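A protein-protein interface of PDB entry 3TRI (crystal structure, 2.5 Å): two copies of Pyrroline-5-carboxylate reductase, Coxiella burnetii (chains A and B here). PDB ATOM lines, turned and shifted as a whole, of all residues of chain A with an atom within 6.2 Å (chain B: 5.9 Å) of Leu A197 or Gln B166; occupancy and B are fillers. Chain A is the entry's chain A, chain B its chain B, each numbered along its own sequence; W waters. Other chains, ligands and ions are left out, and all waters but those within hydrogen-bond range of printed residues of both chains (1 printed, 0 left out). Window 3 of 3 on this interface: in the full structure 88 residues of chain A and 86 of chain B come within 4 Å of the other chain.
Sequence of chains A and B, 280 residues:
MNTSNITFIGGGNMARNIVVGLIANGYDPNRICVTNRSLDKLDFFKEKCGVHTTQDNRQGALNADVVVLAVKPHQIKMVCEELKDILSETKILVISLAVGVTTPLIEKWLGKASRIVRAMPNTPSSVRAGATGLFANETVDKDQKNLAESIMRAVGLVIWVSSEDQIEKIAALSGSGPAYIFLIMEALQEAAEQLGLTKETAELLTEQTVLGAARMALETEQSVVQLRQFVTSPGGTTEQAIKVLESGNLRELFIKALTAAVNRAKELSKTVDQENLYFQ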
ATOM      1  N   GLN A 189      26.354 -18.629  25.705  1.00  0.00           N
ATOM      2  CA  GLN A 189      26.614 -20.064  25.687  1.00  0.00           C
ATOM      3  C   GLN A 189      26.493 -20.674  27.081  1.00  0.00           C
ATOM      4  O   GLN A 189      26.103 -21.830  27.229  1.00  0.00           O
ATOM      5  CB  GLN A 189      27.969 -20.384  25.036  1.00  0.00           C
ATOM      6  CG  GLN A 189      29.181 -19.817  25.747  1.00  0.00           C
ATOM      7  CD  GLN A 189      30.422 -19.829  24.870  1.00  0.00           C
ATOM      8  OE1 GLN A 189      30.331 -19.973  23.649  1.00  0.00           O
ATOM      9  NE2 GLN A 189      31.587 -19.672  25.486  1.00  0.00           N
ATOM     10  N   ALA A 192      22.960 -21.147  27.499  1.00  0.00           N
ATOM     11  CA  ALA A 192      22.578 -22.358  26.787  1.00  0.00           C
ATOM     12  C   ALA A 192      22.963 -23.612  27.572  1.00  0.00           C
ATOM     13  O   ALA A 192      22.259 -24.620  27.537  1.00  0.00           O
ATOM     14  CB  ALA A 192      23.207 -22.378  25.405  1.00  0.00           C
ATOM     15  N   GLU A 193      24.085 -23.550  28.276  1.00  0.00           N
ATOM     16  CA  GLU A 193      24.494 -24.658  29.128  1.00  0.00           C
ATOM     17  C   GLU A 193      23.586 -24.748  30.345  1.00  0.00           C
ATOM     18  O   GLU A 193      23.310 -25.835  30.844  1.00  0.00           O
ATOM     19  CB  GLU A 193      25.943 -24.490  29.575  1.00  0.00           C
ATOM     20  CG  GLU A 193      26.957 -24.646  28.469  1.00  0.00           C
ATOM     21  CD  GLU A 193      28.363 -24.381  28.956  1.00  0.00           C
ATOM     22  OE1 GLU A 193      28.818 -25.099  29.872  1.00  0.00           O
ATOM     23  OE2 GLU A 193      29.005 -23.441  28.438  1.00  0.00           O
ATOM     24  N   GLN A 194      23.123 -23.598  30.816  1.00  0.00           N
ATOM     25  CA  GLN A 194      22.194 -23.564  31.934  1.00  0.00           C
ATOM     26  C   GLN A 194      20.917 -24.323  31.568  1.00  0.00           C
ATOM     27  O   GLN A 194      20.356 -25.042  32.397  1.00  0.00           O
ATOM     28  CB  GLN A 194      21.883 -22.118  32.330  1.00  0.00           C
ATOM     29  CG  GLN A 194      21.095 -21.970  33.626  1.00  0.00           C
ATOM     30  CD  GLN A 194      21.820 -22.547  34.822  1.00  0.00           C
ATOM     31  OE1 GLN A 194      21.664 -23.723  35.146  1.00  0.00           O
ATOM     32  NE2 GLN A 194      22.618 -21.723  35.486  1.00  0.00           N
ATOM     33  N   LEU A 195      20.473 -24.179  30.322  1.00  0.00           N
ATOM     34  CA  LEU A 195      19.278 -24.878  29.850  1.00  0.00           C
ATOM     35  C   LEU A 195      19.520 -26.370  29.661  1.00  0.00           C
ATOM     36  O   LEU A 195      18.572 -27.133  29.474  1.00  0.00           O
ATOM     37  CB  LEU A 195      18.756 -24.285  28.537  1.00  0.00           C
ATOM     38  CG  LEU A 195      18.406 -22.798  28.471  1.00  0.00           C
ATOM     39  CD1 LEU A 195      17.317 -22.596  27.438  1.00  0.00           C
ATOM     40  CD2 LEU A 195      17.969 -22.250  29.818  1.00  0.00           C
ATOM     41  N   GLY A 196      20.780 -26.788  29.692  1.00  0.00           N
ATOM     42  CA  GLY A 196      21.083 -28.204  29.626  1.00  0.00           C
ATOM     43  C   GLY A 196      21.911 -28.693  28.452  1.00  0.00           C
ATOM     44  O   GLY A 196      22.246 -29.877  28.391  1.00  0.00           O
ATOM     45  N   LEU A 197      22.240 -27.806  27.517  1.00  0.00           N
ATOM     46  CA  LEU A 197      23.113 -28.188  26.405  1.00  0.00           C
ATOM     47  C   LEU A 197      24.559 -28.392  26.865  1.00  0.00           C
ATOM     48  O   LEU A 197      25.001 -27.796  27.850  1.00  0.00           O
ATOM     49  CB  LEU A 197      23.067 -27.146  25.289  1.00  0.00           C
ATOM     50  CG  LEU A 197      21.779 -27.070  24.471  1.00  0.00           C
ATOM     51  CD1 LEU A 197      21.845 -25.891  23.520  1.00  0.00           C
ATOM     52  CD2 LEU A 197      21.522 -28.368  23.710  1.00  0.00           C
ATOM     53  N   THR A 198      25.295 -29.237  26.152  1.00  0.00           N
ATOM     54  CA  THR A 198      26.694 -29.481  26.484  1.00  0.00           C
ATOM     55  C   THR A 198      27.543 -28.258  26.167  1.00  0.00           C
ATOM     56  O   THR A 198      27.123 -27.377  25.416  1.00  0.00           O
ATOM     57  CB  THR A 198      27.257 -30.697  25.729  1.00  0.00           C
ATOM     58  OG1 THR A 198      27.281 -30.429  24.321  1.00  0.00           O
ATOM     59  CG2 THR A 198      26.401 -31.918  25.990  1.00  0.00           C
ATOM     60  N   LYS A 199      28.738 -28.212  26.745  1.00  0.00           N
ATOM     61  CA  LYS A 199      29.637 -27.083  26.558  1.00  0.00           C
ATOM     62  C   LYS A 199      30.007 -26.947  25.091  1.00  0.00           C
ATOM     63  O   LYS A 199      30.003 -25.847  24.540  1.00  0.00           O
ATOM     64  CB  LYS A 199      30.902 -27.271  27.396  1.00  0.00           C
ATOM     65  CG  LYS A 199      31.532 -25.979  27.887  1.00  0.00           C
ATOM     66  CD  LYS A 199      32.513 -26.252  29.022  1.00  0.00           C
ATOM     67  CE  LYS A 199      32.938 -24.967  29.717  1.00  0.00           C
ATOM     68  NZ  LYS A 199      31.777 -24.236  30.309  1.00  0.00           N
ATOM     69  N   THR A 201      28.491 -28.100  22.302  1.00  0.00           N
ATOM     70  CA  THR A 201      27.377 -27.715  21.451  1.00  0.00           C
ATOM     71  C   THR A 201      27.006 -26.252  21.670  1.00  0.00           C
ATOM     72  O   THR A 201      26.792 -25.509  20.717  1.00  0.00           O
ATOM     73  CB  THR A 201      26.159 -28.605  21.707  1.00  0.00           C
ATOM     74  OG1 THR A 201      26.505 -29.966  21.431  1.00  0.00           O
ATOM     75  CG2 THR A 201      25.010 -28.198  20.812  1.00  0.00           C
ATOM     76  N   ALA A 202      26.942 -25.843  22.932  1.00  0.00           N
ATOM     77  CA  ALA A 202      26.616 -24.466  23.274  1.00  0.00           C
ATOM     78  C   ALA A 202      27.636 -23.504  22.684  1.00  0.00           C
ATOM     79  O   ALA A 202      27.272 -22.468  22.132  1.00  0.00           O
ATOM     80  CB  ALA A 202      26.536 -24.298  24.779  1.00  0.00           C
ATOM     81  N   LEU A 205      27.384 -23.602  18.599  1.00  0.00           N
ATOM     82  CA  LEU A 205      26.190 -22.940  18.096  1.00  0.00           C
ATOM     83  C   LEU A 205      26.256 -21.443  18.352  1.00  0.00           C
ATOM     84  O   LEU A 205      25.891 -20.648  17.487  1.00  0.00           O
ATOM     85  CB  LEU A 205      24.927 -23.536  18.723  1.00  0.00           C
ATOM     86  CG  LEU A 205      24.634 -24.993  18.371  1.00  0.00           C
ATOM     87  CD1 LEU A 205      23.432 -25.502  19.158  1.00  0.00           C
ATOM     88  CD2 LEU A 205      24.411 -25.141  16.874  1.00  0.00           C
ATOM     89  N   VAL B 161      22.023 -33.925  18.872  1.00  0.00           N
ATOM     90  CA  VAL B 161      21.516 -34.070  20.229  1.00  0.00           C
ATOM     91  C   VAL B 161      21.039 -35.505  20.427  1.00  0.00           C
ATOM     92  O   VAL B 161      20.429 -36.094  19.534  1.00  0.00           O
ATOM     93  CB  VAL B 161      20.350 -33.096  20.520  1.00  0.00           C
ATOM     94  CG1 VAL B 161      20.829 -31.657  20.455  1.00  0.00           C
ATOM     95  CG2 VAL B 161      19.209 -33.324  19.544  1.00  0.00           C
ATOM     96  N   SER B 162      21.323 -36.068  21.598  1.00  0.00           N
ATOM     97  CA  SER B 162      20.944 -37.449  21.893  1.00  0.00           C
ATOM     98  C   SER B 162      19.432 -37.617  22.026  1.00  0.00           C
ATOM     99  O   SER B 162      18.886 -38.656  21.666  1.00  0.00           O
ATOM    100  CB  SER B 162      21.642 -37.947  23.162  1.00  0.00           C
ATOM    101  OG  SER B 162      21.277 -37.157  24.281  1.00  0.00           O
ATOM    102  N   SER B 163      18.760 -36.589  22.541  1.00  0.00           N
ATOM    103  CA  SER B 163      17.309 -36.633  22.715  1.00  0.00           C
ATOM    104  C   SER B 163      16.614 -35.505  21.954  1.00  0.00           C
ATOM    105  O   SER B 163      17.142 -34.397  21.844  1.00  0.00           O
ATOM    106  CB  SER B 163      16.932 -36.583  24.198  1.00  0.00           C
ATOM    107  OG  SER B 163      17.329 -35.358  24.787  1.00  0.00           O
ATOM    108  N   GLU B 164      15.426 -35.798  21.434  1.00  0.00           N
ATOM    109  CA  GLU B 164      14.707 -34.860  20.583  1.00  0.00           C
ATOM    110  C   GLU B 164      14.185 -33.654  21.357  1.00  0.00           C
ATOM    111  O   GLU B 164      13.775 -32.657  20.763  1.00  0.00           O
ATOM    112  CB  GLU B 164      13.558 -35.571  19.858  1.00  0.00           C
ATOM    113  CG  GLU B 164      12.802 -34.698  18.865  1.00  0.00           C
ATOM    114  CD  GLU B 164      11.825 -35.488  18.015  1.00  0.00           C
ATOM    115  OE1 GLU B 164      11.587 -36.671  18.333  1.00  0.00           O
ATOM    116  OE2 GLU B 164      11.300 -34.927  17.027  1.00  0.00           O
ATOM    117  N   ASP B 165      14.205 -33.743  22.683  1.00  0.00           N
ATOM    118  CA  ASP B 165      13.741 -32.636  23.510  1.00  0.00           C
ATOM    119  C   ASP B 165      14.792 -31.529  23.579  1.00  0.00           C
ATOM    120  O   ASP B 165      14.524 -30.430  24.062  1.00  0.00           O
ATOM    121  CB  ASP B 165      13.350 -33.119  24.912  1.00  0.00           C
ATOM    122  CG  ASP B 165      14.506 -33.771  25.658  1.00  0.00           C
ATOM    123  OD1 ASP B 165      15.656 -33.295  25.527  1.00  0.00           O
ATOM    124  OD2 ASP B 165      14.260 -34.759  26.386  1.00  0.00           O
ATOM    125  N   GLN B 166      15.989 -31.822  23.088  1.00  0.00           N
ATOM    126  CA  GLN B 166      17.052 -30.830  23.080  1.00  0.00           C
ATOM    127  C   GLN B 166      16.950 -29.937  21.849  1.00  0.00           C
ATOM    128  O   GLN B 166      17.587 -28.883  21.784  1.00  0.00           O
ATOM    129  CB  GLN B 166      18.423 -31.502  23.159  1.00  0.00           C
ATOM    130  CG  GLN B 166      18.542 -32.500  24.299  1.00  0.00           C
ATOM    131  CD  GLN B 166      19.972 -32.942  24.549  1.00  0.00           C
ATOM    132  OE1 GLN B 166      20.908 -32.150  24.445  1.00  0.00           O
ATOM    133  NE2 GLN B 166      20.146 -34.215  24.886  1.00  0.00           N
ATOM    134  N   ILE B 167      16.134 -30.352  20.884  1.00  0.00           N
ATOM    135  CA  ILE B 167      15.915 -29.554  19.679  1.00  0.00           C
ATOM    136  C   ILE B 167      15.321 -28.188  20.019  1.00  0.00           C
ATOM    137  O   ILE B 167      15.718 -27.172  19.450  1.00  0.00           O
ATOM    138  CB  ILE B 167      15.020 -30.287  18.653  1.00  0.00           C
ATOM    139  CG1 ILE B 167      15.823 -31.364  17.921  1.00  0.00           C
ATOM    140  CG2 ILE B 167      14.448 -29.315  17.644  1.00  0.00           C
ATOM    141  CD1 ILE B 167      16.965 -30.823  17.084  1.00  0.00           C
ATOM    142  N   GLU B 168      14.381 -28.165  20.958  1.00  0.00           N
ATOM    143  CA  GLU B 168      13.788 -26.908  21.402  1.00  0.00           C
ATOM    144  C   GLU B 168      14.823 -25.994  22.061  1.00  0.00           C
ATOM    145  O   GLU B 168      14.651 -24.774  22.097  1.00  0.00           O
ATOM    146  CB  GLU B 168      12.618 -27.164  22.356  1.00  0.00           C
ATOM    147  CG  GLU B 168      11.319 -27.569  21.670  1.00  0.00           C
ATOM    148  CD  GLU B 168      11.315 -29.010  21.191  1.00  0.00           C
ATOM    149  OE1 GLU B 168      12.204 -29.783  21.609  1.00  0.00           O
ATOM    150  OE2 GLU B 168      10.419 -29.366  20.394  1.00  0.00           O
ATOM    151  N   LYS B 169      15.893 -26.587  22.583  1.00  0.00           N
ATOM    152  CA  LYS B 169      16.985 -25.812  23.167  1.00  0.00           C
ATOM    153  C   LYS B 169      17.894 -25.278  22.069  1.00  0.00           C
ATOM    154  O   LYS B 169      18.451 -24.189  22.187  1.00  0.00           O
ATOM    155  CB  LYS B 169      17.781 -26.657  24.161  1.00  0.00           C
ATOM    156  CG  LYS B 169      16.919 -27.295  25.239  1.00  0.00           C
ATOM    157  CD  LYS B 169      17.760 -27.946  26.321  1.00  0.00           C
ATOM    158  CE  LYS B 169      16.896 -28.813  27.210  1.00  0.00           C
ATOM    159  NZ  LYS B 169      17.668 -29.479  28.289  1.00  0.00           N
ATOM    160  N   ILE B 170      18.033 -26.049  20.997  1.00  0.00           N
ATOM    161  CA  ILE B 170      18.739 -25.584  19.812  1.00  0.00           C
ATOM    162  C   ILE B 170      18.002 -24.400  19.208  1.00  0.00           C
ATOM    163  O   ILE B 170      18.599 -23.361  18.913  1.00  0.00           O
ATOM    164  CB  ILE B 170      18.836 -26.683  18.738  1.00  0.00           C
ATOM    165  CG1 ILE B 170      19.545 -27.919  19.299  1.00  0.00           C
ATOM    166  CG2 ILE B 170      19.538 -26.149  17.493  1.00  0.00           C
ATOM    167  CD1 ILE B 170      20.845 -27.607  20.005  1.00  0.00           C
ATOM    168  N   ALA B 171      16.696 -24.567  19.024  1.00  0.00           N
ATOM    169  CA  ALA B 171      15.861 -23.519  18.456  1.00  0.00           C
ATOM    170  C   ALA B 171      16.024 -22.223  19.235  1.00  0.00           C
ATOM    171  O   ALA B 171      16.127 -21.148  18.651  1.00  0.00           O
ATOM    172  CB  ALA B 171      14.405 -23.949  18.445  1.00  0.00           C
ATOM    173  N   LEU B 173      18.581 -21.348  21.110  1.00  0.00           N
ATOM    174  CA  LEU B 173      19.945 -20.842  21.000  1.00  0.00           C
ATOM    175  C   LEU B 173      20.318 -20.394  19.581  1.00  0.00           C
ATOM    176  O   LEU B 173      20.481 -19.204  19.326  1.00  0.00           O
ATOM    177  CB  LEU B 173      20.949 -21.881  21.507  1.00  0.00           C
ATOM    178  CG  LEU B 173      22.416 -21.497  21.295  1.00  0.00           C
ATOM    179  CD1 LEU B 173      22.676 -20.101  21.848  1.00  0.00           C
ATOM    180  CD2 LEU B 173      23.362 -22.526  21.915  1.00  0.00           C
HETATM  181  O   HOH W   1      23.653 -31.011  23.905  1.00  0.00           O
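The side-chain amino group (NZ) of Lys B169 lies within hydrogen-bond range of the backbone carbonyl oxygen (O) of Leu A195 (2.8 Å).
Hydrophobic or aromatic side chains of chain B that line the printed part of chain A: Ile B170 and Leu B173. Of the 12 printed residues of chain A, 6 touch a printed residue of chain B. Hydrophobic or aromatic side chains of chain A that line the printed part of chain B: Ala A192, Leu A197 and Leu A205.
Of the printed residues of chain B, Ala A192 touches Leu B173. Leu A197 touches just these residues of chain B: Gln B166 (3.9 Å) and Ile B170 (3.8 Å). Gln B166 touches just one residue of chain A: Leu A197 (3.9 Å). Printed residues of chain A within 4 Å of Lys B169: Leu A195 (2.8 Å) and Gly A196 (3.9 Å). Printed residues of chain A within 4 Å of Leu B173: Ala A192, Ala A202 and Leu A205. The nearest residue of chain A that does not touch Gln B166 is Gly A196 (4.7 Å). The nearest printed residue of chain B that does not touch Ala A192 is Lys B169 (5.7 Å).
Among the printed residues, merely in contact across the chains: Leu A205 with Ile B170 (3.4 Å), Ala A192 with Leu B173 (3.5 Å), Leu A205 with Leu B173 (3.7 Å), Leu A197 with Ile B170 (3.8 Å), Gly A196 with Lys B169 (3.9 Å), Leu A197 with Gln B166 (3.9 Å) and Ala A202 with Leu B173 (3.9 Å).
No position is printed for both chains. Of the 8 pairs that touch across the chains among the printed residues, none has its exchanged pair printed and touching as well.
Water W1 lies within hydrogen-bond range of the side-chain amide oxygen of Gln B166 (3.0 Å) and the backbone NH of Thr A198 (3.3 Å).
OG of Ser B163 lies within hydrogen-bond range of NE2 of Gln B166 (3.0 Å). The backbone carbonyl oxygen (O) of Ala A192 is in hydrogen-bond range of the backbone NH (N) of Leu A197 (3.2 Å). NE2 of Gln B166 lies within hydrogen-bond range of OG of Ser B162 (3.2 Å).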
